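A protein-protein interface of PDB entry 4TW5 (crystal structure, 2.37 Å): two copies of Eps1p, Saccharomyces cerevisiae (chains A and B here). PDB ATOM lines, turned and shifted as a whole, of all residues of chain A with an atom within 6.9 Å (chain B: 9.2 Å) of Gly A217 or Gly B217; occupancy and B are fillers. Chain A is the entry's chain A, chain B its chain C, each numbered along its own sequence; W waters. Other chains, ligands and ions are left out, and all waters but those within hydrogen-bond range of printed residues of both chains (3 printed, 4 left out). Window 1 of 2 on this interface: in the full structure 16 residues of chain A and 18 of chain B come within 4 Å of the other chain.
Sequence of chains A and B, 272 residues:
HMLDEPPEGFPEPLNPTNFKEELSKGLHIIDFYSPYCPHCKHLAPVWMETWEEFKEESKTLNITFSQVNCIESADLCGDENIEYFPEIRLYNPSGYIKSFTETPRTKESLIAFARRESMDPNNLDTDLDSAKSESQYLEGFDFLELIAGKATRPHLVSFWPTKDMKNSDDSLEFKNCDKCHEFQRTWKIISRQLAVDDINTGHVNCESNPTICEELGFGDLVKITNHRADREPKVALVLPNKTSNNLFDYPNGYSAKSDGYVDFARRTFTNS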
ATOM      1  N   ILE A 212      28.702   7.848 -15.795  1.00  0.00           N
ATOM      2  CA  ILE A 212      28.292   6.959 -16.864  1.00  0.00           C
ATOM      3  C   ILE A 212      27.171   7.543 -17.729  1.00  0.00           C
ATOM      4  O   ILE A 212      27.271   7.568 -18.944  1.00  0.00           O
ATOM      5  CB  ILE A 212      27.862   5.623 -16.296  1.00  0.00           C
ATOM      6  CG1 ILE A 212      29.075   4.967 -15.629  1.00  0.00           C
ATOM      7  CG2 ILE A 212      27.292   4.763 -17.389  1.00  0.00           C
ATOM      8  CD1 ILE A 212      28.784   3.635 -15.013  1.00  0.00           C
ATOM      9  N   CYS A 213      26.127   8.064 -17.113  1.00  0.00           N
ATOM     10  CA  CYS A 213      25.020   8.627 -17.882  1.00  0.00           C
ATOM     11  C   CYS A 213      25.412   9.911 -18.662  1.00  0.00           C
ATOM     12  O   CYS A 213      24.873  10.208 -19.736  1.00  0.00           O
ATOM     13  CB  CYS A 213      23.848   8.896 -16.944  1.00  0.00           C
ATOM     14  SG  CYS A 213      22.968   7.370 -16.424  1.00  0.00           S
ATOM     15  N   GLU A 214      26.343  10.678 -18.114  1.00  0.00           N
ATOM     16  CA  GLU A 214      26.823  11.862 -18.808  1.00  0.00           C
ATOM     17  C   GLU A 214      27.627  11.460 -20.036  1.00  0.00           C
ATOM     18  O   GLU A 214      27.392  11.964 -21.130  1.00  0.00           O
ATOM     19  CB  GLU A 214      27.623  12.754 -17.844  1.00  0.00           C
ATOM     20  CG  GLU A 214      26.676  13.638 -17.006  1.00  0.00           C
ATOM     21  CD  GLU A 214      27.297  14.181 -15.714  1.00  0.00           C
ATOM     22  OE1 GLU A 214      28.482  13.918 -15.420  1.00  0.00           O
ATOM     23  OE2 GLU A 214      26.567  14.854 -14.971  1.00  0.00           O
ATOM     24  N   GLU A 215      28.529  10.502 -19.861  1.00  0.00           N
ATOM     25  CA  GLU A 215      29.379  10.051 -20.948  1.00  0.00           C
ATOM     26  C   GLU A 215      28.592   9.416 -22.093  1.00  0.00           C
ATOM     27  O   GLU A 215      28.921   9.635 -23.256  1.00  0.00           O
ATOM     28  CB  GLU A 215      30.395   9.064 -20.395  1.00  0.00           C
ATOM     29  CG  GLU A 215      31.487   9.711 -19.574  1.00  0.00           C
ATOM     30  CD  GLU A 215      32.498   8.708 -19.058  1.00  0.00           C
ATOM     31  OE1 GLU A 215      32.185   7.498 -19.067  1.00  0.00           O
ATOM     32  OE2 GLU A 215      33.610   9.126 -18.668  1.00  0.00           O
ATOM     33  N   LEU A 216      27.518   8.702 -21.758  1.00  0.00           N
ATOM     34  CA  LEU A 216      26.663   8.011 -22.716  1.00  0.00           C
ATOM     35  C   LEU A 216      25.692   8.919 -23.447  1.00  0.00           C
ATOM     36  O   LEU A 216      24.966   8.475 -24.342  1.00  0.00           O
ATOM     37  CB  LEU A 216      25.851   6.936 -22.007  1.00  0.00           C
ATOM     38  CG  LEU A 216      26.611   5.717 -21.505  1.00  0.00           C
ATOM     39  CD1 LEU A 216      25.619   4.700 -21.033  1.00  0.00           C
ATOM     40  CD2 LEU A 216      27.470   5.159 -22.584  1.00  0.00           C
ATOM     41  N   GLY A 217      25.616  10.176 -23.026  1.00  0.00           N
ATOM     42  CA  GLY A 217      24.656  11.069 -23.628  1.00  0.00           C
ATOM     43  C   GLY A 217      23.293  11.071 -22.981  1.00  0.00           C
ATOM     44  O   GLY A 217      22.323  11.432 -23.656  1.00  0.00           O
ATOM     45  N   PHE A 218      23.200  10.638 -21.715  1.00  0.00           N
ATOM     46  CA  PHE A 218      21.938  10.706 -20.968  1.00  0.00           C
ATOM     47  C   PHE A 218      22.033  11.679 -19.781  1.00  0.00           C
ATOM     48  O   PHE A 218      21.305  11.553 -18.778  1.00  0.00           O
ATOM     49  CB  PHE A 218      21.523   9.308 -20.465  1.00  0.00           C
ATOM     50  CG  PHE A 218      21.534   8.257 -21.531  1.00  0.00           C
ATOM     51  CD1 PHE A 218      21.102   8.551 -22.814  1.00  0.00           C
ATOM     52  CD2 PHE A 218      22.003   6.975 -21.253  1.00  0.00           C
ATOM     53  CE1 PHE A 218      21.121   7.580 -23.805  1.00  0.00           C
ATOM     54  CE2 PHE A 218      22.040   6.008 -22.229  1.00  0.00           C
ATOM     55  CZ  PHE A 218      21.595   6.306 -23.513  1.00  0.00           C
ATOM     56  N   GLY A 219      22.912  12.665 -19.933  1.00  0.00           N
ATOM     57  CA  GLY A 219      23.240  13.593 -18.881  1.00  0.00           C
ATOM     58  C   GLY A 219      22.057  14.374 -18.348  1.00  0.00           C
ATOM     59  O   GLY A 219      22.087  14.808 -17.203  1.00  0.00           O
ATOM     60  N   ASP A 220      21.012  14.509 -19.162  1.00  0.00           N
ATOM     61  CA  ASP A 220      19.817  15.237 -18.778  1.00  0.00           C
ATOM     62  C   ASP A 220      18.984  14.466 -17.714  1.00  0.00           C
ATOM     63  O   ASP A 220      18.101  15.034 -17.082  1.00  0.00           O
ATOM     64  CB  ASP A 220      18.977  15.545 -20.021  1.00  0.00           C
ATOM     65  CG  ASP A 220      18.774  14.343 -20.907  1.00  0.00           C
ATOM     66  OD1 ASP A 220      19.738  13.579 -21.131  1.00  0.00           O
ATOM     67  OD2 ASP A 220      17.657  14.200 -21.448  1.00  0.00           O
ATOM     68  N   LEU A 221      19.256  13.173 -17.545  1.00  0.00           N
ATOM     69  CA  LEU A 221      18.566  12.370 -16.543  1.00  0.00           C
ATOM     70  C   LEU A 221      19.260  12.410 -15.190  1.00  0.00           C
ATOM     71  O   LEU A 221      18.706  11.970 -14.187  1.00  0.00           O
ATOM     72  CB  LEU A 221      18.455  10.902 -17.000  1.00  0.00           C
ATOM     73  CG  LEU A 221      17.905  10.585 -18.394  1.00  0.00           C
ATOM     74  CD1 LEU A 221      17.548   9.086 -18.519  1.00  0.00           C
ATOM     75  CD2 LEU A 221      16.764  11.471 -18.815  1.00  0.00           C
ATOM     76  N   ARG A 228      15.372  22.649 -18.964  1.00  0.00           N
ATOM     77  CA  ARG A 228      14.577  21.635 -19.651  1.00  0.00           C
ATOM     78  C   ARG A 228      13.353  21.340 -18.818  1.00  0.00           C
ATOM     79  O   ARG A 228      13.457  20.893 -17.669  1.00  0.00           O
ATOM     80  CB  ARG A 228      15.355  20.344 -19.910  1.00  0.00           C
ATOM     81  CG  ARG A 228      16.461  20.484 -20.925  1.00  0.00           C
ATOM     82  CD  ARG A 228      17.090  19.133 -21.180  1.00  0.00           C
ATOM     83  NE  ARG A 228      18.146  19.225 -22.178  1.00  0.00           N
ATOM     84  CZ  ARG A 228      17.927  19.328 -23.480  1.00  0.00           C
ATOM     85  NH1 ARG A 228      16.687  19.376 -23.951  1.00  0.00           N
ATOM     86  NH2 ARG A 228      18.954  19.407 -24.297  1.00  0.00           N
ATOM     87  N   LYS A 234      15.607   6.853 -21.369  1.00  0.00           N
ATOM     88  CA  LYS A 234      16.287   6.473 -22.606  1.00  0.00           C
ATOM     89  C   LYS A 234      16.495   4.972 -22.660  1.00  0.00           C
ATOM     90  O   LYS A 234      16.549   4.321 -21.627  1.00  0.00           O
ATOM     91  CB  LYS A 234      17.621   7.200 -22.736  1.00  0.00           C
ATOM     92  CG  LYS A 234      17.455   8.708 -22.730  1.00  0.00           C
ATOM     93  CD  LYS A 234      16.749   9.199 -23.969  1.00  0.00           C
ATOM     94  CE  LYS A 234      16.869  10.723 -24.026  1.00  0.00           C
ATOM     95  NZ  LYS A 234      16.350  11.307 -25.298  1.00  0.00           N
ATOM     96  N   ASP A 249      21.924   3.271 -29.380  1.00  0.00           N
ATOM     97  CA  ASP A 249      20.717   3.966 -28.895  1.00  0.00           C
ATOM     98  C   ASP A 249      19.483   3.619 -29.703  1.00  0.00           C
ATOM     99  O   ASP A 249      19.545   3.431 -30.923  1.00  0.00           O
ATOM    100  CB  ASP A 249      20.864   5.488 -28.937  1.00  0.00           C
ATOM    101  CG  ASP A 249      21.763   6.023 -27.849  1.00  0.00           C
ATOM    102  OD1 ASP A 249      22.362   5.215 -27.107  1.00  0.00           O
ATOM    103  OD2 ASP A 249      21.819   7.265 -27.697  1.00  0.00           O
ATOM    104  N   PHE B 159      24.928  21.523 -31.987  1.00  0.00           N
ATOM    105  CA  PHE B 159      25.999  21.031 -31.115  1.00  0.00           C
ATOM    106  C   PHE B 159      26.836  19.961 -31.856  1.00  0.00           C
ATOM    107  O   PHE B 159      26.276  19.025 -32.440  1.00  0.00           O
ATOM    108  CB  PHE B 159      25.400  20.463 -29.803  1.00  0.00           C
ATOM    109  CG  PHE B 159      24.626  21.501 -28.983  1.00  0.00           C
ATOM    110  CD1 PHE B 159      23.327  21.871 -29.341  1.00  0.00           C
ATOM    111  CD2 PHE B 159      25.206  22.098 -27.873  1.00  0.00           C
ATOM    112  CE1 PHE B 159      22.637  22.833 -28.612  1.00  0.00           C
ATOM    113  CE2 PHE B 159      24.550  23.037 -27.157  1.00  0.00           C
ATOM    114  CZ  PHE B 159      23.243  23.420 -27.504  1.00  0.00           C
ATOM    115  N   CYS B 206      31.250  20.898 -28.692  1.00  0.00           N
ATOM    116  CA  CYS B 206      31.097  20.144 -27.455  1.00  0.00           C
ATOM    117  C   CYS B 206      32.427  19.705 -26.887  1.00  0.00           C
ATOM    118  O   CYS B 206      32.560  19.632 -25.661  1.00  0.00           O
ATOM    119  CB  CYS B 206      30.207  18.946 -27.672  1.00  0.00           C
ATOM    120  SG  CYS B 206      28.532  19.412 -27.661  1.00  0.00           S
ATOM    121  N   PRO B 210      32.861  20.442 -22.331  1.00  0.00           N
ATOM    122  CA  PRO B 210      32.418  19.095 -21.905  1.00  0.00           C
ATOM    123  C   PRO B 210      31.258  19.093 -20.871  1.00  0.00           C
ATOM    124  O   PRO B 210      30.247  18.398 -21.059  1.00  0.00           O
ATOM    125  CB  PRO B 210      33.693  18.467 -21.311  1.00  0.00           C
ATOM    126  CG  PRO B 210      34.618  19.650 -21.027  1.00  0.00           C
ATOM    127  CD  PRO B 210      34.275  20.717 -22.010  1.00  0.00           C
ATOM    128  N   THR B 211      31.364  19.895 -19.824  1.00  0.00           N
ATOM    129  CA  THR B 211      30.343  19.830 -18.785  1.00  0.00           C
ATOM    130  C   THR B 211      28.989  20.291 -19.311  1.00  0.00           C
ATOM    131  O   THR B 211      27.970  19.628 -19.100  1.00  0.00           O
ATOM    132  CB  THR B 211      30.761  20.647 -17.556  1.00  0.00           C
ATOM    133  OG1 THR B 211      31.904  20.002 -16.980  1.00  0.00           O
ATOM    134  CG2 THR B 211      29.661  20.679 -16.526  1.00  0.00           C
ATOM    135  N   ILE B 212      28.977  21.387 -20.052  1.00  0.00           N
ATOM    136  CA  ILE B 212      27.725  21.837 -20.630  1.00  0.00           C
ATOM    137  C   ILE B 212      27.047  20.808 -21.527  1.00  0.00           C
ATOM    138  O   ILE B 212      25.864  20.518 -21.341  1.00  0.00           O
ATOM    139  CB  ILE B 212      27.933  23.112 -21.420  1.00  0.00           C
ATOM    140  CG1 ILE B 212      28.272  24.237 -20.419  1.00  0.00           C
ATOM    141  CG2 ILE B 212      26.670  23.430 -22.202  1.00  0.00           C
ATOM    142  CD1 ILE B 212      28.529  25.579 -21.007  1.00  0.00           C
ATOM    143  N   CYS B 213      27.792  20.243 -22.472  1.00  0.00           N
ATOM    144  CA  CYS B 213      27.205  19.281 -23.405  1.00  0.00           C
ATOM    145  C   CYS B 213      26.843  17.983 -22.693  1.00  0.00           C
ATOM    146  O   CYS B 213      25.814  17.394 -22.991  1.00  0.00           O
ATOM    147  CB  CYS B 213      28.155  19.001 -24.594  1.00  0.00           C
ATOM    148  SG  CYS B 213      28.222  20.375 -25.832  1.00  0.00           S
ATOM    149  N   GLU B 214      27.631  17.590 -21.701  1.00  0.00           N
ATOM    150  CA  GLU B 214      27.286  16.414 -20.907  1.00  0.00           C
ATOM    151  C   GLU B 214      25.993  16.639 -20.141  1.00  0.00           C
ATOM    152  O   GLU B 214      25.109  15.786 -20.158  1.00  0.00           O
ATOM    153  CB  GLU B 214      28.407  16.050 -19.926  1.00  0.00           C
ATOM    154  CG  GLU B 214      29.532  15.210 -20.542  1.00  0.00           C
ATOM    155  CD  GLU B 214      30.805  15.177 -19.698  1.00  0.00           C
ATOM    156  OE1 GLU B 214      30.850  15.810 -18.627  1.00  0.00           O
ATOM    157  OE2 GLU B 214      31.770  14.503 -20.104  1.00  0.00           O
ATOM    158  N   GLU B 215      25.860  17.795 -19.490  1.00  0.00           N
ATOM    159  CA  GLU B 215      24.634  18.077 -18.723  1.00  0.00           C
ATOM    160  C   GLU B 215      23.410  18.236 -19.643  1.00  0.00           C
ATOM    161  O   GLU B 215      22.274  17.870 -19.266  1.00  0.00           O
ATOM    162  CB  GLU B 215      24.828  19.304 -17.829  1.00  0.00           C
ATOM    163  CG  GLU B 215      25.857  18.999 -16.719  1.00  0.00           C
ATOM    164  CD  GLU B 215      26.027  20.090 -15.662  1.00  0.00           C
ATOM    165  OE1 GLU B 215      25.506  21.234 -15.843  1.00  0.00           O
ATOM    166  OE2 GLU B 215      26.739  19.788 -14.664  1.00  0.00           O
ATOM    167  N   LEU B 216      23.647  18.720 -20.865  1.00  0.00           N
ATOM    168  CA  LEU B 216      22.556  18.958 -21.812  1.00  0.00           C
ATOM    169  C   LEU B 216      22.024  17.667 -22.414  1.00  0.00           C
ATOM    170  O   LEU B 216      21.032  17.692 -23.147  1.00  0.00           O
ATOM    171  CB  LEU B 216      23.017  19.891 -22.946  1.00  0.00           C
ATOM    172  CG  LEU B 216      23.193  21.386 -22.681  1.00  0.00           C
ATOM    173  CD1 LEU B 216      23.556  22.201 -23.946  1.00  0.00           C
ATOM    174  CD2 LEU B 216      21.883  21.873 -22.141  1.00  0.00           C
ATOM    175  N   GLY B 217      22.697  16.553 -22.134  1.00  0.00           N
ATOM    176  CA  GLY B 217      22.347  15.280 -22.734  1.00  0.00           C
ATOM    177  C   GLY B 217      23.063  15.049 -24.063  1.00  0.00           C
ATOM    178  O   GLY B 217      22.658  14.194 -24.840  1.00  0.00           O
ATOM    179  N   PHE B 218      24.131  15.809 -24.316  1.00  0.00           N
ATOM    180  CA  PHE B 218      24.971  15.615 -25.513  1.00  0.00           C
ATOM    181  C   PHE B 218      26.377  15.141 -25.185  1.00  0.00           C
ATOM    182  O   PHE B 218      27.307  15.447 -25.919  1.00  0.00           O
ATOM    183  CB  PHE B 218      25.121  16.899 -26.336  1.00  0.00           C
ATOM    184  CG  PHE B 218      23.837  17.580 -26.659  1.00  0.00           C
ATOM    185  CD1 PHE B 218      22.711  16.859 -26.964  1.00  0.00           C
ATOM    186  CD2 PHE B 218      23.770  18.955 -26.684  1.00  0.00           C
ATOM    187  CE1 PHE B 218      21.531  17.494 -27.266  1.00  0.00           C
ATOM    188  CE2 PHE B 218      22.602  19.571 -26.988  1.00  0.00           C
ATOM    189  CZ  PHE B 218      21.476  18.829 -27.293  1.00  0.00           C
ATOM    190  N   GLY B 219      26.548  14.410 -24.096  1.00  0.00           N
ATOM    191  CA  GLY B 219      27.871  13.961 -23.699  1.00  0.00           C
ATOM    192  C   GLY B 219      28.651  13.108 -24.722  1.00  0.00           C
ATOM    193  O   GLY B 219      29.852  12.965 -24.587  1.00  0.00           O
ATOM    194  N   ASP B 220      27.961  12.500 -25.683  1.00  0.00           N
ATOM    195  CA  ASP B 220      28.592  11.620 -26.670  1.00  0.00           C
ATOM    196  C   ASP B 220      29.354  12.418 -27.704  1.00  0.00           C
ATOM    197  O   ASP B 220      30.197  11.868 -28.408  1.00  0.00           O
ATOM    198  CB  ASP B 220      27.564  10.687 -27.334  1.00  0.00           C
ATOM    199  CG  ASP B 220      26.294  11.390 -27.737  1.00  0.00           C
ATOM    200  OD1 ASP B 220      25.795  12.222 -26.952  1.00  0.00           O
ATOM    201  OD2 ASP B 220      25.714  11.044 -28.785  1.00  0.00           O
ATOM    202  N   LEU B 221      29.072  13.720 -27.779  1.00  0.00           N
ATOM    203  CA  LEU B 221      29.789  14.576 -28.689  1.00  0.00           C
ATOM    204  C   LEU B 221      31.048  15.090 -28.048  1.00  0.00           C
ATOM    205  O   LEU B 221      31.840  15.702 -28.700  1.00  0.00           O
ATOM    206  CB  LEU B 221      28.933  15.738 -29.156  1.00  0.00           C
ATOM    207  CG  LEU B 221      27.561  15.379 -29.736  1.00  0.00           C
ATOM    208  CD1 LEU B 221      27.000  16.595 -30.439  1.00  0.00           C
ATOM    209  CD2 LEU B 221      27.662  14.175 -30.695  1.00  0.00           C
ATOM    210  N   VAL B 222      31.222  14.887 -26.752  1.00  0.00           N
ATOM    211  CA  VAL B 222      32.345  15.527 -26.067  1.00  0.00           C
ATOM    212  C   VAL B 222      33.645  14.844 -26.351  1.00  0.00           C
ATOM    213  O   VAL B 222      34.672  15.487 -26.494  1.00  0.00           O
ATOM    214  CB  VAL B 222      32.148  15.549 -24.527  1.00  0.00           C
ATOM    215  CG1 VAL B 222      33.454  15.930 -23.807  1.00  0.00           C
ATOM    216  CG2 VAL B 222      31.025  16.517 -24.143  1.00  0.00           C
ATOM    217  N   LYS B 223      33.550  13.518 -26.410  1.00  0.00           N
ATOM    218  CA  LYS B 223      34.666  12.587 -26.373  1.00  0.00           C
ATOM    219  C   LYS B 223      34.520  11.327 -27.257  1.00  0.00           C
ATOM    220  O   LYS B 223      33.435  10.763 -27.422  1.00  0.00           O
ATOM    221  CB  LYS B 223      34.864  12.156 -24.913  1.00  0.00           C
ATOM    222  CG  LYS B 223      36.045  11.255 -24.648  1.00  0.00           C
ATOM    223  CD  LYS B 223      36.338  11.205 -23.161  1.00  0.00           C
ATOM    224  CE  LYS B 223      36.725  12.592 -22.664  1.00  0.00           C
ATOM    225  NZ  LYS B 223      37.150  12.590 -21.233  1.00  0.00           N
ATOM    226  N   THR B 225      34.655   7.471 -27.843  1.00  0.00           N
ATOM    227  CA  THR B 225      34.544   6.217 -27.093  1.00  0.00           C
ATOM    228  C   THR B 225      34.489   5.019 -28.068  1.00  0.00           C
ATOM    229  O   THR B 225      34.041   5.149 -29.212  1.00  0.00           O
ATOM    230  CB  THR B 225      33.309   6.190 -26.197  1.00  0.00           C
ATOM    231  OG1 THR B 225      32.134   6.308 -27.008  1.00  0.00           O
ATOM    232  CG2 THR B 225      33.352   7.333 -25.173  1.00  0.00           C
ATOM    233  N   HIS B 227      32.688   2.348 -27.757  1.00  0.00           N
ATOM    234  CA  HIS B 227      31.438   1.598 -27.686  1.00  0.00           C
ATOM    235  C   HIS B 227      30.359   2.144 -28.625  1.00  0.00           C
ATOM    236  O   HIS B 227      29.496   1.392 -29.078  1.00  0.00           O
ATOM    237  CB  HIS B 227      30.909   1.527 -26.242  1.00  0.00           C
ATOM    238  CG  HIS B 227      30.911   2.832 -25.505  1.00  0.00           C
ATOM    239  ND1 HIS B 227      30.270   3.958 -25.974  1.00  0.00           N
ATOM    240  CD2 HIS B 227      31.439   3.172 -24.306  1.00  0.00           C
ATOM    241  CE1 HIS B 227      30.417   4.941 -25.103  1.00  0.00           C
ATOM    242  NE2 HIS B 227      31.126   4.491 -24.083  1.00  0.00           N
ATOM    243  N   ARG B 228      30.412   3.433 -28.941  1.00  0.00           N
ATOM    244  CA  ARG B 228      29.487   4.014 -29.916  1.00  0.00           C
ATOM    245  C   ARG B 228      30.112   4.076 -31.312  1.00  0.00           C
ATOM    246  O   ARG B 228      31.123   4.748 -31.513  1.00  0.00           O
ATOM    247  CB  ARG B 228      29.058   5.425 -29.476  1.00  0.00           C
ATOM    248  CG  ARG B 228      28.170   5.433 -28.248  1.00  0.00           C
ATOM    249  CD  ARG B 228      27.709   6.830 -27.825  1.00  0.00           C
ATOM    250  NE  ARG B 228      26.789   6.680 -26.700  1.00  0.00           N
ATOM    251  CZ  ARG B 228      25.511   6.356 -26.846  1.00  0.00           C
ATOM    252  NH1 ARG B 228      24.996   6.231 -28.059  1.00  0.00           N
ATOM    253  NH2 ARG B 228      24.740   6.185 -25.796  1.00  0.00           N
ATOM    254  N   GLU B 232      25.960  11.878 -34.064  1.00  0.00           N
ATOM    255  CA  GLU B 232      25.443  12.809 -35.021  1.00  0.00           C
ATOM    256  C   GLU B 232      25.287  14.148 -34.304  1.00  0.00           C
ATOM    257  O   GLU B 232      25.170  14.175 -33.073  1.00  0.00           O
ATOM    258  CB  GLU B 232      24.135  12.283 -35.595  1.00  0.00           C
ATOM    259  CG  GLU B 232      22.994  12.196 -34.603  1.00  0.00           C
ATOM    260  CD  GLU B 232      21.740  11.650 -35.251  1.00  0.00           C
ATOM    261  OE1 GLU B 232      21.867  10.738 -36.097  1.00  0.00           O
ATOM    262  OE2 GLU B 232      20.643  12.176 -34.977  1.00  0.00           O
ATOM    263  N   LYS B 234      23.657  17.420 -32.664  1.00  0.00           N
ATOM    264  CA  LYS B 234      22.378  17.672 -32.030  1.00  0.00           C
ATOM    265  C   LYS B 234      21.902  19.094 -32.201  1.00  0.00           C
ATOM    266  O   LYS B 234      22.693  20.034 -32.299  1.00  0.00           O
ATOM    267  CB  LYS B 234      22.447  17.339 -30.543  1.00  0.00           C
ATOM    268  CG  LYS B 234      22.553  15.881 -30.261  1.00  0.00           C
ATOM    269  CD  LYS B 234      21.204  15.289 -30.662  1.00  0.00           C
ATOM    270  CE  LYS B 234      20.980  13.869 -30.188  1.00  0.00           C
ATOM    271  NZ  LYS B 234      19.558  13.510 -30.507  1.00  0.00           N
ATOM    272  N   VAL B 235      20.583  19.246 -32.143  1.00  0.00           N
ATOM    273  CA  VAL B 235      19.952  20.529 -32.338  1.00  0.00           C
ATOM    274  C   VAL B 235      19.006  20.886 -31.178  1.00  0.00           C
ATOM    275  O   VAL B 235      18.217  20.059 -30.722  1.00  0.00           O
ATOM    276  CB  VAL B 235      19.149  20.542 -33.658  1.00  0.00           C
ATOM    277  CG1 VAL B 235      18.493  21.918 -33.859  1.00  0.00           C
ATOM    278  CG2 VAL B 235      20.047  20.207 -34.834  1.00  0.00           C
ATOM    279  N   LEU B 247      14.449  25.683 -23.182  1.00  0.00           N
ATOM    280  CA  LEU B 247      15.311  24.830 -24.018  1.00  0.00           C
ATOM    281  C   LEU B 247      14.607  23.557 -24.445  1.00  0.00           C
ATOM    282  O   LEU B 247      14.302  22.714 -23.638  1.00  0.00           O
ATOM    283  CB  LEU B 247      16.615  24.488 -23.293  1.00  0.00           C
ATOM    284  CG  LEU B 247      17.658  23.725 -24.120  1.00  0.00           C
ATOM    285  CD1 LEU B 247      18.152  24.516 -25.287  1.00  0.00           C
ATOM    286  CD2 LEU B 247      18.839  23.417 -23.231  1.00  0.00           C
ATOM    287  N   ASP B 249      14.846  20.339 -27.207  1.00  0.00           N
ATOM    288  CA  ASP B 249      15.540  19.530 -28.225  1.00  0.00           C
ATOM    289  C   ASP B 249      14.701  19.307 -29.481  1.00  0.00           C
ATOM    290  O   ASP B 249      13.481  19.134 -29.388  1.00  0.00           O
ATOM    291  CB  ASP B 249      15.944  18.162 -27.641  1.00  0.00           C
ATOM    292  CG  ASP B 249      17.186  18.237 -26.763  1.00  0.00           C
ATOM    293  OD1 ASP B 249      17.761  19.341 -26.633  1.00  0.00           O
ATOM    294  OD2 ASP B 249      17.584  17.199 -26.184  1.00  0.00           O
HETATM  295  O   HOH W   1      19.628  19.212 -19.222  1.00  0.00           O
HETATM  296  O   HOH W   2      23.323   9.248 -26.696  1.00  0.00           O
HETATM  297  O   HOH W   3      29.406   7.944 -25.415  1.00  0.00           O
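Printed residues of chain A that touch a printed residue of chain B: Glu A214, Glu A215, Leu A216, Gly A217, Phe A218, Gly A219, Asp A220, Arg A228 and Asp A249.
Hydrophobic or aromatic side chains of chain A within 4 Å of the printed part of chain B: Leu A216 and Phe A218.
Of the 24 printed residues of chain B, 10 touch a printed residue of chain A.
Along chain B the printed residues that touch a printed residue of chain A span positions 214 to 249.
Among the printed residues, 19 pairs touch across the chains.
Among the printed residues, Asp or Glu carboxylates within 4 Å of a Lys or Arg side-chain nitrogen of the other chain: Arg A228 with Asp B249 (2.6 Å) and Asp A249 with Arg B228 (2.9 Å).
Gly B219 touches Glu A214.
Gly B219 touches Glu A215.
Asp B220 touches Glu A215 (N to O, 3.9 Å).
Leu A216 touches His B227.
Gly B219 touches Gly A217.
Asp B220 touches Gly A217.
Phe A218 touches Arg B228.
O of Glu B214 touches CA of Gly A219, 3.2 Å away.
Glu B215 touches Gly A219.
CZ of Phe B218 touches NH2 of Arg A228 (3.96 Å).
Glu B214 touches its own counterpart, Glu A214.
Glu A214 touches Gly B219, and with the chains exchanged Gly A219 touches Glu B214.
Glu A215 touches Gly B219, and with the chains exchanged Gly A219 touches Glu B215.
Gly A217 touches Gly B219, and with the chains exchanged Gly A219 touches Gly B217.
Positions printed for both chains: 212, 213, 214, 215, 216, 217, 218, 219, 220, 221, 228, 234 and 249.
O of Leu A216 is in hydrogen-bond range of NH2 of Arg B228, 2.7 Å away.
O of Leu B216 is in hydrogen-bond range of NH2 of Arg A228.
The side-chain carboxylate (OD1) of Asp B249 lies within salt-bridge range of the guanidinium group (NH2) of Arg A228, 2.6 Å away.
The side-chain carboxylate (OD1) of Asp A249 is in salt-bridge range of the guanidinium group (NH2) of Arg B228 (2.9 Å).
O of Gly A217 sits close to O of Gly B217.
The backbone NH (N) of Phe A218 lies within hydrogen-bond range of the backbone carbonyl oxygen (O) of Cys A213 (2.6 Å).
The backbone NH (N) of Gly A219 is in hydrogen-bond range of the backbone carbonyl oxygen (O) of Cys A213, at 3.1 Å.
The backbone carbonyl oxygen (O) of Cys B213 is in hydrogen-bond range of the backbone NH (N) of Phe B218, 2.7 Å away.
O of Cys B213 is in hydrogen-bond range of N of Gly B219 (3.3 Å).
A ring nitrogen (ND1) of His B227 sits close to the side-chain hydroxyl (OG1) of Thr B225, at 3.2 Å.
SG of Cys B213 forms a disulfide with SG of Cys B206.
Water W2 lies within hydrogen-bond range of OD2 of Asp A249, O of Leu A216 and NH2 of Arg B228.
Water W3 lies within hydrogen-bond range of O of Glu A215 (2.8 Å) and NE of Arg B228 (3.2 Å).
Water W1 bridges O of Glu B215 and NE of Arg A228.
Printed residues of chain B within 4 Å of Glu A214: Glu B214 (3.9 Å) and Gly B219 (3.3 Å).
Printed residues of chain B within 4 Å of Leu A216: His B227 and Arg B228.
Of chain B, only Gly B217 (3.0 Å), Gly B219 (3.9 Å) and Asp B220 (3.7 Å) come within 4 Å of Gly A217.
Of chain A, only Gly A217, Gly A219 and Asp A220 come within 4 Å of Gly B217.
The nearest residue of chain A that does not touch Gly B217 is Phe A218 (4.7 Å).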
